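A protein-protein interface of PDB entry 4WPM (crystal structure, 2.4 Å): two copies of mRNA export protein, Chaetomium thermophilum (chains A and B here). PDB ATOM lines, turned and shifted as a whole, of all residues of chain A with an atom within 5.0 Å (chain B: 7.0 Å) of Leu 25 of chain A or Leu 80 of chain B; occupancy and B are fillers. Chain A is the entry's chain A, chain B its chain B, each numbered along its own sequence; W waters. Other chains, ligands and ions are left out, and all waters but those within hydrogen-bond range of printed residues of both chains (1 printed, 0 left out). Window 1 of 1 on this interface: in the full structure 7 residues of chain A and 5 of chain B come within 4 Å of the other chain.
The side-chain carboxylate of Asp 65 of chain A is in hydrogen-bond range of the backbone NH of Glu 96 of chain B, 2.7 Å away. The backbone carbonyl oxygen of Leu 80 of chain B is in hydrogen-bond range of the side-chain hydroxyl of Tyr 66 of chain A (3.4 Å).
O of Leu 25 of chain A sits at hydrogen-bond distance from N of Thr 93 of chain A (2.9 Å). The side-chain carboxylate (OE1) of Glu 95 of chain B is in salt-bridge range of the side-chain amino group (NZ) of Lys 23 of chain B, at 3.8 Å.
Leu 25 of chain A touches Leu 80 of chain B (CD2 to CD1, 3.6 Å). Asp 65 of chain A touches Leu 80 of chain B. Glu 95 of chain B touches Asp 65 of chain A (CA to OD2, 3.3 Å). OH of Tyr 66 of chain A touches N of Arg 81 of chain B, at 3.8 Å. NE2 of Gln 77 of chain B touches CG2 of Thr 93 of chain A, 3.7 Å away.
Leu 25 of chain A touches just one residue of chain B: Leu 80 (3.6 Å). Leu 27 of chain A touches none of the printed residues of chain B. Of the printed residues of chain B, Tyr 66 of chain A touches Leu 80 (3.4 Å) and Arg 81 (3.8 Å). Printed residues of chain B within 4 Å of Thr 93 of chain A: Gln 77 (3.7 Å). Of the printed residues of chain A, Gln 77 of chain B touches Thr 93 (3.7 Å). Leu 80 of chain B touches three residues of chain A. Of the printed residues of chain A, Arg 81 of chain B touches Tyr 66. Printed residues of chain A within 4 Å of Glu 96 of chain B: Asp 65. The nearest residue of chain B that does not touch Leu 25 of chain A is Gln 77 of chain B (4.8 Å). The nearest printed residue of chain B that does not touch Thr 93 of chain A is Arg 81 of chain B (6.3 Å).
Of the 10 printed residues of chain A, 4 touch a printed residue of chain B. Hydrophobic or aromatic side chains of chain B within 4 Å of the printed part of chain A: Leu 80. Among the printed residues, 7 pairs touch across the chains.
Position printed for both chains: 23. Of the 7 pairs that touch across the chains among the printed residues, none has its exchanged pair printed and touching as well.
Water W1 bridges OD1 of Asp 65 of chain A (2.6 Å) and OE2 of Glu 95 of chain B (2.8 Å).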
ATOM      1  N   LYS A  23       6.633   9.712 -23.982  1.00  0.00           N
ATOM      2  CA  LYS A  23       5.604  10.689 -23.640  1.00  0.00           C
ATOM      3  C   LYS A  23       4.549  10.050 -22.744  1.00  0.00           C
ATOM      4  O   LYS A  23       4.032   8.975 -23.050  1.00  0.00           O
ATOM      5  CB  LYS A  23       4.955  11.247 -24.908  1.00  0.00           C
ATOM      6  CG  LYS A  23       5.897  12.080 -25.766  1.00  0.00           C
ATOM      7  CD  LYS A  23       5.206  12.671 -26.995  1.00  0.00           C
ATOM      8  CE  LYS A  23       4.046  13.593 -26.642  1.00  0.00           C
ATOM      9  NZ  LYS A  23       3.425  14.176 -27.864  1.00  0.00           N
ATOM     10  N   ILE A  24       4.236  10.723 -21.640  1.00  0.00           N
ATOM     11  CA  ILE A  24       3.246  10.236 -20.683  1.00  0.00           C
ATOM     12  C   ILE A  24       2.097  11.226 -20.536  1.00  0.00           C
ATOM     13  O   ILE A  24       2.317  12.416 -20.309  1.00  0.00           O
ATOM     14  CB  ILE A  24       3.876   9.986 -19.298  1.00  0.00           C
ATOM     15  CG1 ILE A  24       5.049   9.009 -19.410  1.00  0.00           C
ATOM     16  CG2 ILE A  24       2.832   9.459 -18.317  1.00  0.00           C
ATOM     17  CD1 ILE A  24       5.881   8.899 -18.150  1.00  0.00           C
ATOM     18  N   LEU A  25       0.875  10.717 -20.659  1.00  0.00           N
ATOM     19  CA  LEU A  25      -0.331  11.529 -20.553  1.00  0.00           C
ATOM     20  C   LEU A  25      -1.205  11.043 -19.401  1.00  0.00           C
ATOM     21  O   LEU A  25      -1.307   9.839 -19.165  1.00  0.00           O
ATOM     22  CB  LEU A  25      -1.116  11.481 -21.865  1.00  0.00           C
ATOM     23  CG  LEU A  25      -2.278  12.459 -22.042  1.00  0.00           C
ATOM     24  CD1 LEU A  25      -1.819  13.908 -21.939  1.00  0.00           C
ATOM     25  CD2 LEU A  25      -2.961  12.201 -23.375  1.00  0.00           C
ATOM     26  N   GLY A  26      -1.830  11.980 -18.691  1.00  0.00           N
ATOM     27  CA  GLY A  26      -2.779  11.645 -17.641  1.00  0.00           C
ATOM     28  C   GLY A  26      -2.380  12.106 -16.250  1.00  0.00           C
ATOM     29  O   GLY A  26      -3.136  11.923 -15.295  1.00  0.00           O
ATOM     30  N   LEU A  27      -1.197  12.700 -16.123  1.00  0.00           N
ATOM     31  CA  LEU A  27      -0.728  13.178 -14.826  1.00  0.00           C
ATOM     32  C   LEU A  27      -1.567  14.360 -14.351  1.00  0.00           C
ATOM     33  O   LEU A  27      -1.802  14.525 -13.156  1.00  0.00           O
ATOM     34  CB  LEU A  27       0.749  13.577 -14.891  1.00  0.00           C
ATOM     35  CG  LEU A  27       1.373  14.026 -13.566  1.00  0.00           C
ATOM     36  CD1 LEU A  27       1.372  12.895 -12.545  1.00  0.00           C
ATOM     37  CD2 LEU A  27       2.785  14.548 -13.780  1.00  0.00           C
ATOM     38  N   ASP A  65       0.293  18.998 -20.997  1.00  0.00           N
ATOM     39  CA  ASP A  65      -0.342  17.903 -20.273  1.00  0.00           C
ATOM     40  C   ASP A  65       0.558  16.671 -20.251  1.00  0.00           C
ATOM     41  O   ASP A  65       0.230  15.667 -19.616  1.00  0.00           O
ATOM     42  CB  ASP A  65      -1.691  17.548 -20.901  1.00  0.00           C
ATOM     43  CG  ASP A  65      -2.648  18.721 -20.933  1.00  0.00           C
ATOM     44  OD1 ASP A  65      -2.397  19.718 -20.223  1.00  0.00           O
ATOM     45  OD2 ASP A  65      -3.659  18.640 -21.661  1.00  0.00           O
ATOM     46  N   TYR A  66       1.694  16.752 -20.941  1.00  0.00           N
ATOM     47  CA  TYR A  66       2.573  15.601 -21.104  1.00  0.00           C
ATOM     48  C   TYR A  66       3.755  15.611 -20.145  1.00  0.00           C
ATOM     49  O   TYR A  66       4.224  16.670 -19.722  1.00  0.00           O
ATOM     50  CB  TYR A  66       3.107  15.543 -22.538  1.00  0.00           C
ATOM     51  CG  TYR A  66       2.098  15.084 -23.564  1.00  0.00           C
ATOM     52  CD1 TYR A  66       1.805  13.736 -23.719  1.00  0.00           C
ATOM     53  CD2 TYR A  66       1.447  15.995 -24.383  1.00  0.00           C
ATOM     54  CE1 TYR A  66       0.888  13.309 -24.658  1.00  0.00           C
ATOM     55  CE2 TYR A  66       0.527  15.577 -25.326  1.00  0.00           C
ATOM     56  CZ  TYR A  66       0.252  14.232 -25.459  1.00  0.00           C
ATOM     57  OH  TYR A  66      -0.662  13.808 -26.395  1.00  0.00           O
ATOM     58  N   THR A  91      -5.833   7.462 -15.533  1.00  0.00           N
ATOM     59  CA  THR A  91      -5.309   6.502 -16.497  1.00  0.00           C
ATOM     60  C   THR A  91      -4.123   7.093 -17.249  1.00  0.00           C
ATOM     61  O   THR A  91      -4.206   8.195 -17.793  1.00  0.00           O
ATOM     62  CB  THR A  91      -6.390   6.073 -17.511  1.00  0.00           C
ATOM     63  OG1 THR A  91      -7.504   5.498 -16.819  1.00  0.00           O
ATOM     64  CG2 THR A  91      -5.834   5.056 -18.503  1.00  0.00           C
ATOM     65  N   LEU A  92      -3.020   6.349 -17.275  1.00  0.00           N
ATOM     66  CA  LEU A  92      -1.808   6.787 -17.953  1.00  0.00           C
ATOM     67  C   LEU A  92      -1.741   6.264 -19.385  1.00  0.00           C
ATOM     68  O   LEU A  92      -1.988   5.084 -19.635  1.00  0.00           O
ATOM     69  CB  LEU A  92      -0.565   6.332 -17.182  1.00  0.00           C
ATOM     70  CG  LEU A  92      -0.295   6.967 -15.812  1.00  0.00           C
ATOM     71  CD1 LEU A  92       1.069   6.529 -15.300  1.00  0.00           C
ATOM     72  CD2 LEU A  92      -0.386   8.488 -15.853  1.00  0.00           C
ATOM     73  N   THR A  93      -1.409   7.153 -20.317  1.00  0.00           N
ATOM     74  CA  THR A  93      -1.127   6.766 -21.694  1.00  0.00           C
ATOM     75  C   THR A  93       0.361   6.971 -21.936  1.00  0.00           C
ATOM     76  O   THR A  93       0.837   8.108 -21.980  1.00  0.00           O
ATOM     77  CB  THR A  93      -1.944   7.591 -22.708  1.00  0.00           C
ATOM     78  OG1 THR A  93      -3.335   7.535 -22.368  1.00  0.00           O
ATOM     79  CG2 THR A  93      -1.745   7.061 -24.122  1.00  0.00           C
ATOM     80  N   ILE B  22     -11.472  20.861 -24.520  1.00  0.00           N
ATOM     81  CA  ILE B  22     -10.125  21.127 -25.011  1.00  0.00           C
ATOM     82  C   ILE B  22      -9.908  22.625 -25.197  1.00  0.00           C
ATOM     83  O   ILE B  22     -10.752  23.317 -25.769  1.00  0.00           O
ATOM     84  CB  ILE B  22      -9.860  20.407 -26.354  1.00  0.00           C
ATOM     85  CG1 ILE B  22     -10.032  18.893 -26.205  1.00  0.00           C
ATOM     86  CG2 ILE B  22      -8.470  20.741 -26.887  1.00  0.00           C
ATOM     87  CD1 ILE B  22      -9.036  18.237 -25.266  1.00  0.00           C
ATOM     88  N   LYS B  23      -8.768  23.114 -24.713  1.00  0.00           N
ATOM     89  CA  LYS B  23      -8.369  24.503 -24.910  1.00  0.00           C
ATOM     90  C   LYS B  23      -7.198  24.588 -25.880  1.00  0.00           C
ATOM     91  O   LYS B  23      -6.218  23.852 -25.744  1.00  0.00           O
ATOM     92  CB  LYS B  23      -7.979  25.162 -23.586  1.00  0.00           C
ATOM     93  CG  LYS B  23      -9.115  25.313 -22.585  1.00  0.00           C
ATOM     94  CD  LYS B  23      -8.690  26.111 -21.348  1.00  0.00           C
ATOM     95  CE  LYS B  23      -7.406  25.600 -20.702  1.00  0.00           C
ATOM     96  NZ  LYS B  23      -6.976  26.480 -19.581  1.00  0.00           N
ATOM     97  N   ASP B  75     -11.697  11.668 -29.258  1.00  0.00           N
ATOM     98  CA  ASP B  75     -11.373  12.891 -29.989  1.00  0.00           C
ATOM     99  C   ASP B  75     -10.356  13.742 -29.234  1.00  0.00           C
ATOM    100  O   ASP B  75      -9.489  14.371 -29.841  1.00  0.00           O
ATOM    101  CB  ASP B  75     -12.640  13.709 -30.254  1.00  0.00           C
ATOM    102  CG  ASP B  75     -13.530  13.086 -31.314  1.00  0.00           C
ATOM    103  OD1 ASP B  75     -13.065  12.176 -32.034  1.00  0.00           O
ATOM    104  OD2 ASP B  75     -14.700  13.507 -31.426  1.00  0.00           O
ATOM    105  N   ALA B  76     -10.470  13.758 -27.909  1.00  0.00           N
ATOM    106  CA  ALA B  76      -9.593  14.574 -27.077  1.00  0.00           C
ATOM    107  C   ALA B  76      -8.142  14.128 -27.212  1.00  0.00           C
ATOM    108  O   ALA B  76      -7.229  14.953 -27.236  1.00  0.00           O
ATOM    109  CB  ALA B  76     -10.034  14.506 -25.623  1.00  0.00           C
ATOM    110  N   GLN B  77      -7.939  12.818 -27.303  1.00  0.00           N
ATOM    111  CA  GLN B  77      -6.600  12.255 -27.424  1.00  0.00           C
ATOM    112  C   GLN B  77      -5.980  12.642 -28.762  1.00  0.00           C
ATOM    113  O   GLN B  77      -4.787  12.930 -28.848  1.00  0.00           O
ATOM    114  CB  GLN B  77      -6.636  10.733 -27.280  1.00  0.00           C
ATOM    115  CG  GLN B  77      -5.270  10.115 -27.026  1.00  0.00           C
ATOM    116  CD  GLN B  77      -5.324   8.607 -26.880  1.00  0.00           C
ATOM    117  OE1 GLN B  77      -6.402   8.015 -26.815  1.00  0.00           O
ATOM    118  NE2 GLN B  77      -4.157   7.978 -26.824  1.00  0.00           N
ATOM    119  N   HIS B  78      -6.807  12.642 -29.802  1.00  0.00           N
ATOM    120  CA  HIS B  78      -6.355  12.956 -31.151  1.00  0.00           C
ATOM    121  C   HIS B  78      -5.901  14.407 -31.254  1.00  0.00           C
ATOM    122  O   HIS B  78      -4.925  14.715 -31.937  1.00  0.00           O
ATOM    123  CB  HIS B  78      -7.480  12.695 -32.153  1.00  0.00           C
ATOM    124  CG  HIS B  78      -8.000  11.292 -32.122  1.00  0.00           C
ATOM    125  ND1 HIS B  78      -7.233  10.221 -31.716  1.00  0.00           N
ATOM    126  CD2 HIS B  78      -9.220  10.787 -32.427  1.00  0.00           C
ATOM    127  CE1 HIS B  78      -7.954   9.116 -31.782  1.00  0.00           C
ATOM    128  NE2 HIS B  78      -9.164   9.433 -32.207  1.00  0.00           N
ATOM    129  N   LEU B  79      -6.620  15.296 -30.577  1.00  0.00           N
ATOM    130  CA  LEU B  79      -6.268  16.711 -30.549  1.00  0.00           C
ATOM    131  C   LEU B  79      -4.973  16.958 -29.779  1.00  0.00           C
ATOM    132  O   LEU B  79      -4.152  17.784 -30.178  1.00  0.00           O
ATOM    133  CB  LEU B  79      -7.407  17.527 -29.937  1.00  0.00           C
ATOM    134  CG  LEU B  79      -8.644  17.706 -30.822  1.00  0.00           C
ATOM    135  CD1 LEU B  79      -9.792  18.297 -30.022  1.00  0.00           C
ATOM    136  CD2 LEU B  79      -8.333  18.577 -32.032  1.00  0.00           C
ATOM    137  N   LEU B  80      -4.796  16.241 -28.673  1.00  0.00           N
ATOM    138  CA  LEU B  80      -3.613  16.406 -27.834  1.00  0.00           C
ATOM    139  C   LEU B  80      -2.346  15.990 -28.576  1.00  0.00           C
ATOM    140  O   LEU B  80      -1.260  16.503 -28.312  1.00  0.00           O
ATOM    141  CB  LEU B  80      -3.753  15.585 -26.550  1.00  0.00           C
ATOM    142  CG  LEU B  80      -4.688  16.146 -25.476  1.00  0.00           C
ATOM    143  CD1 LEU B  80      -4.891  15.126 -24.371  1.00  0.00           C
ATOM    144  CD2 LEU B  80      -4.146  17.445 -24.899  1.00  0.00           C
ATOM    145  N   ARG B  81      -2.501  15.055 -29.505  1.00  0.00           N
ATOM    146  CA  ARG B  81      -1.395  14.583 -30.326  1.00  0.00           C
ATOM    147  C   ARG B  81      -0.862  15.711 -31.206  1.00  0.00           C
ATOM    148  O   ARG B  81       0.324  15.755 -31.530  1.00  0.00           O
ATOM    149  CB  ARG B  81      -1.854  13.406 -31.184  1.00  0.00           C
ATOM    150  CG  ARG B  81      -1.852  12.080 -30.445  1.00  0.00           C
ATOM    151  CD  ARG B  81      -2.350  10.951 -31.324  1.00  0.00           C
ATOM    152  NE  ARG B  81      -2.675   9.764 -30.538  1.00  0.00           N
ATOM    153  CZ  ARG B  81      -2.978   8.578 -31.056  1.00  0.00           C
ATOM    154  NH1 ARG B  81      -3.011   8.409 -32.371  1.00  0.00           N
ATOM    155  NH2 ARG B  81      -3.260   7.561 -30.254  1.00  0.00           N
ATOM    156  N   LEU B  82      -1.754  16.620 -31.587  1.00  0.00           N
ATOM    157  CA  LEU B  82      -1.407  17.725 -32.477  1.00  0.00           C
ATOM    158  C   LEU B  82      -0.744  18.885 -31.735  1.00  0.00           C
ATOM    159  O   LEU B  82      -0.425  19.912 -32.337  1.00  0.00           O
ATOM    160  CB  LEU B  82      -2.659  18.225 -33.202  1.00  0.00           C
ATOM    161  CG  LEU B  82      -3.469  17.167 -33.955  1.00  0.00           C
ATOM    162  CD1 LEU B  82      -4.703  17.790 -34.588  1.00  0.00           C
ATOM    163  CD2 LEU B  82      -2.620  16.469 -35.008  1.00  0.00           C
ATOM    164  N   ASN B  83      -0.545  18.723 -30.431  1.00  0.00           N
ATOM    165  CA  ASN B  83       0.111  19.746 -29.623  1.00  0.00           C
ATOM    166  C   ASN B  83       1.537  20.013 -30.087  1.00  0.00           C
ATOM    167  O   ASN B  83       2.317  19.084 -30.294  1.00  0.00           O
ATOM    168  CB  ASN B  83       0.109  19.340 -28.147  1.00  0.00           C
ATOM    169  CG  ASN B  83       0.827  20.344 -27.266  1.00  0.00           C
ATOM    170  OD1 ASN B  83       0.270  21.382 -26.907  1.00  0.00           O
ATOM    171  ND2 ASN B  83       2.070  20.039 -26.912  1.00  0.00           N
ATOM    172  N   GLY B  84       1.872  21.292 -30.234  1.00  0.00           N
ATOM    173  CA  GLY B  84       3.202  21.700 -30.650  1.00  0.00           C
ATOM    174  C   GLY B  84       3.351  21.937 -32.142  1.00  0.00           C
ATOM    175  O   GLY B  84       4.392  22.420 -32.588  1.00  0.00           O
ATOM    176  N   ILE B  94      -2.274  22.751 -27.128  1.00  0.00           N
ATOM    177  CA  ILE B  94      -3.543  22.073 -26.881  1.00  0.00           C
ATOM    178  C   ILE B  94      -3.535  21.424 -25.504  1.00  0.00           C
ATOM    179  O   ILE B  94      -2.598  20.709 -25.144  1.00  0.00           O
ATOM    180  CB  ILE B  94      -3.856  21.010 -27.957  1.00  0.00           C
ATOM    181  CG1 ILE B  94      -4.061  21.672 -29.322  1.00  0.00           C
ATOM    182  CG2 ILE B  94      -5.163  20.296 -27.647  1.00  0.00           C
ATOM    183  CD1 ILE B  94      -2.805  22.020 -30.081  1.00  0.00           C
ATOM    184  N   GLU B  95      -4.596  21.684 -24.744  1.00  0.00           N
ATOM    185  CA  GLU B  95      -4.697  21.223 -23.368  1.00  0.00           C
ATOM    186  C   GLU B  95      -6.075  20.641 -23.090  1.00  0.00           C
ATOM    187  O   GLU B  95      -7.084  21.138 -23.594  1.00  0.00           O
ATOM    188  CB  GLU B  95      -4.444  22.381 -22.401  1.00  0.00           C
ATOM    189  CG  GLU B  95      -3.140  23.123 -22.620  1.00  0.00           C
ATOM    190  CD  GLU B  95      -2.960  24.267 -21.642  1.00  0.00           C
ATOM    191  OE1 GLU B  95      -3.978  24.846 -21.205  1.00  0.00           O
ATOM    192  OE2 GLU B  95      -1.803  24.593 -21.314  1.00  0.00           O
ATOM    193  N   GLU B  96      -6.110  19.585 -22.284  1.00  0.00           N
ATOM    194  CA  GLU B  96      -7.364  19.044 -21.781  1.00  0.00           C
ATOM    195  C   GLU B  96      -7.708  19.735 -20.467  1.00  0.00           C
ATOM    196  O   GLU B  96      -6.815  20.060 -19.684  1.00  0.00           O
ATOM    197  CB  GLU B  96      -7.266  17.531 -21.587  1.00  0.00           C
ATOM    198  CG  GLU B  96      -8.601  16.860 -21.316  1.00  0.00           C
ATOM    199  CD  GLU B  96      -8.464  15.381 -21.018  1.00  0.00           C
ATOM    200  OE1 GLU B  96      -7.567  14.736 -21.602  1.00  0.00           O
ATOM    201  OE2 GLU B  96      -9.255  14.861 -20.202  1.00  0.00           O
HETATM  202  O   HOH W   1      -1.348  22.043 -20.127  1.00  0.00           O
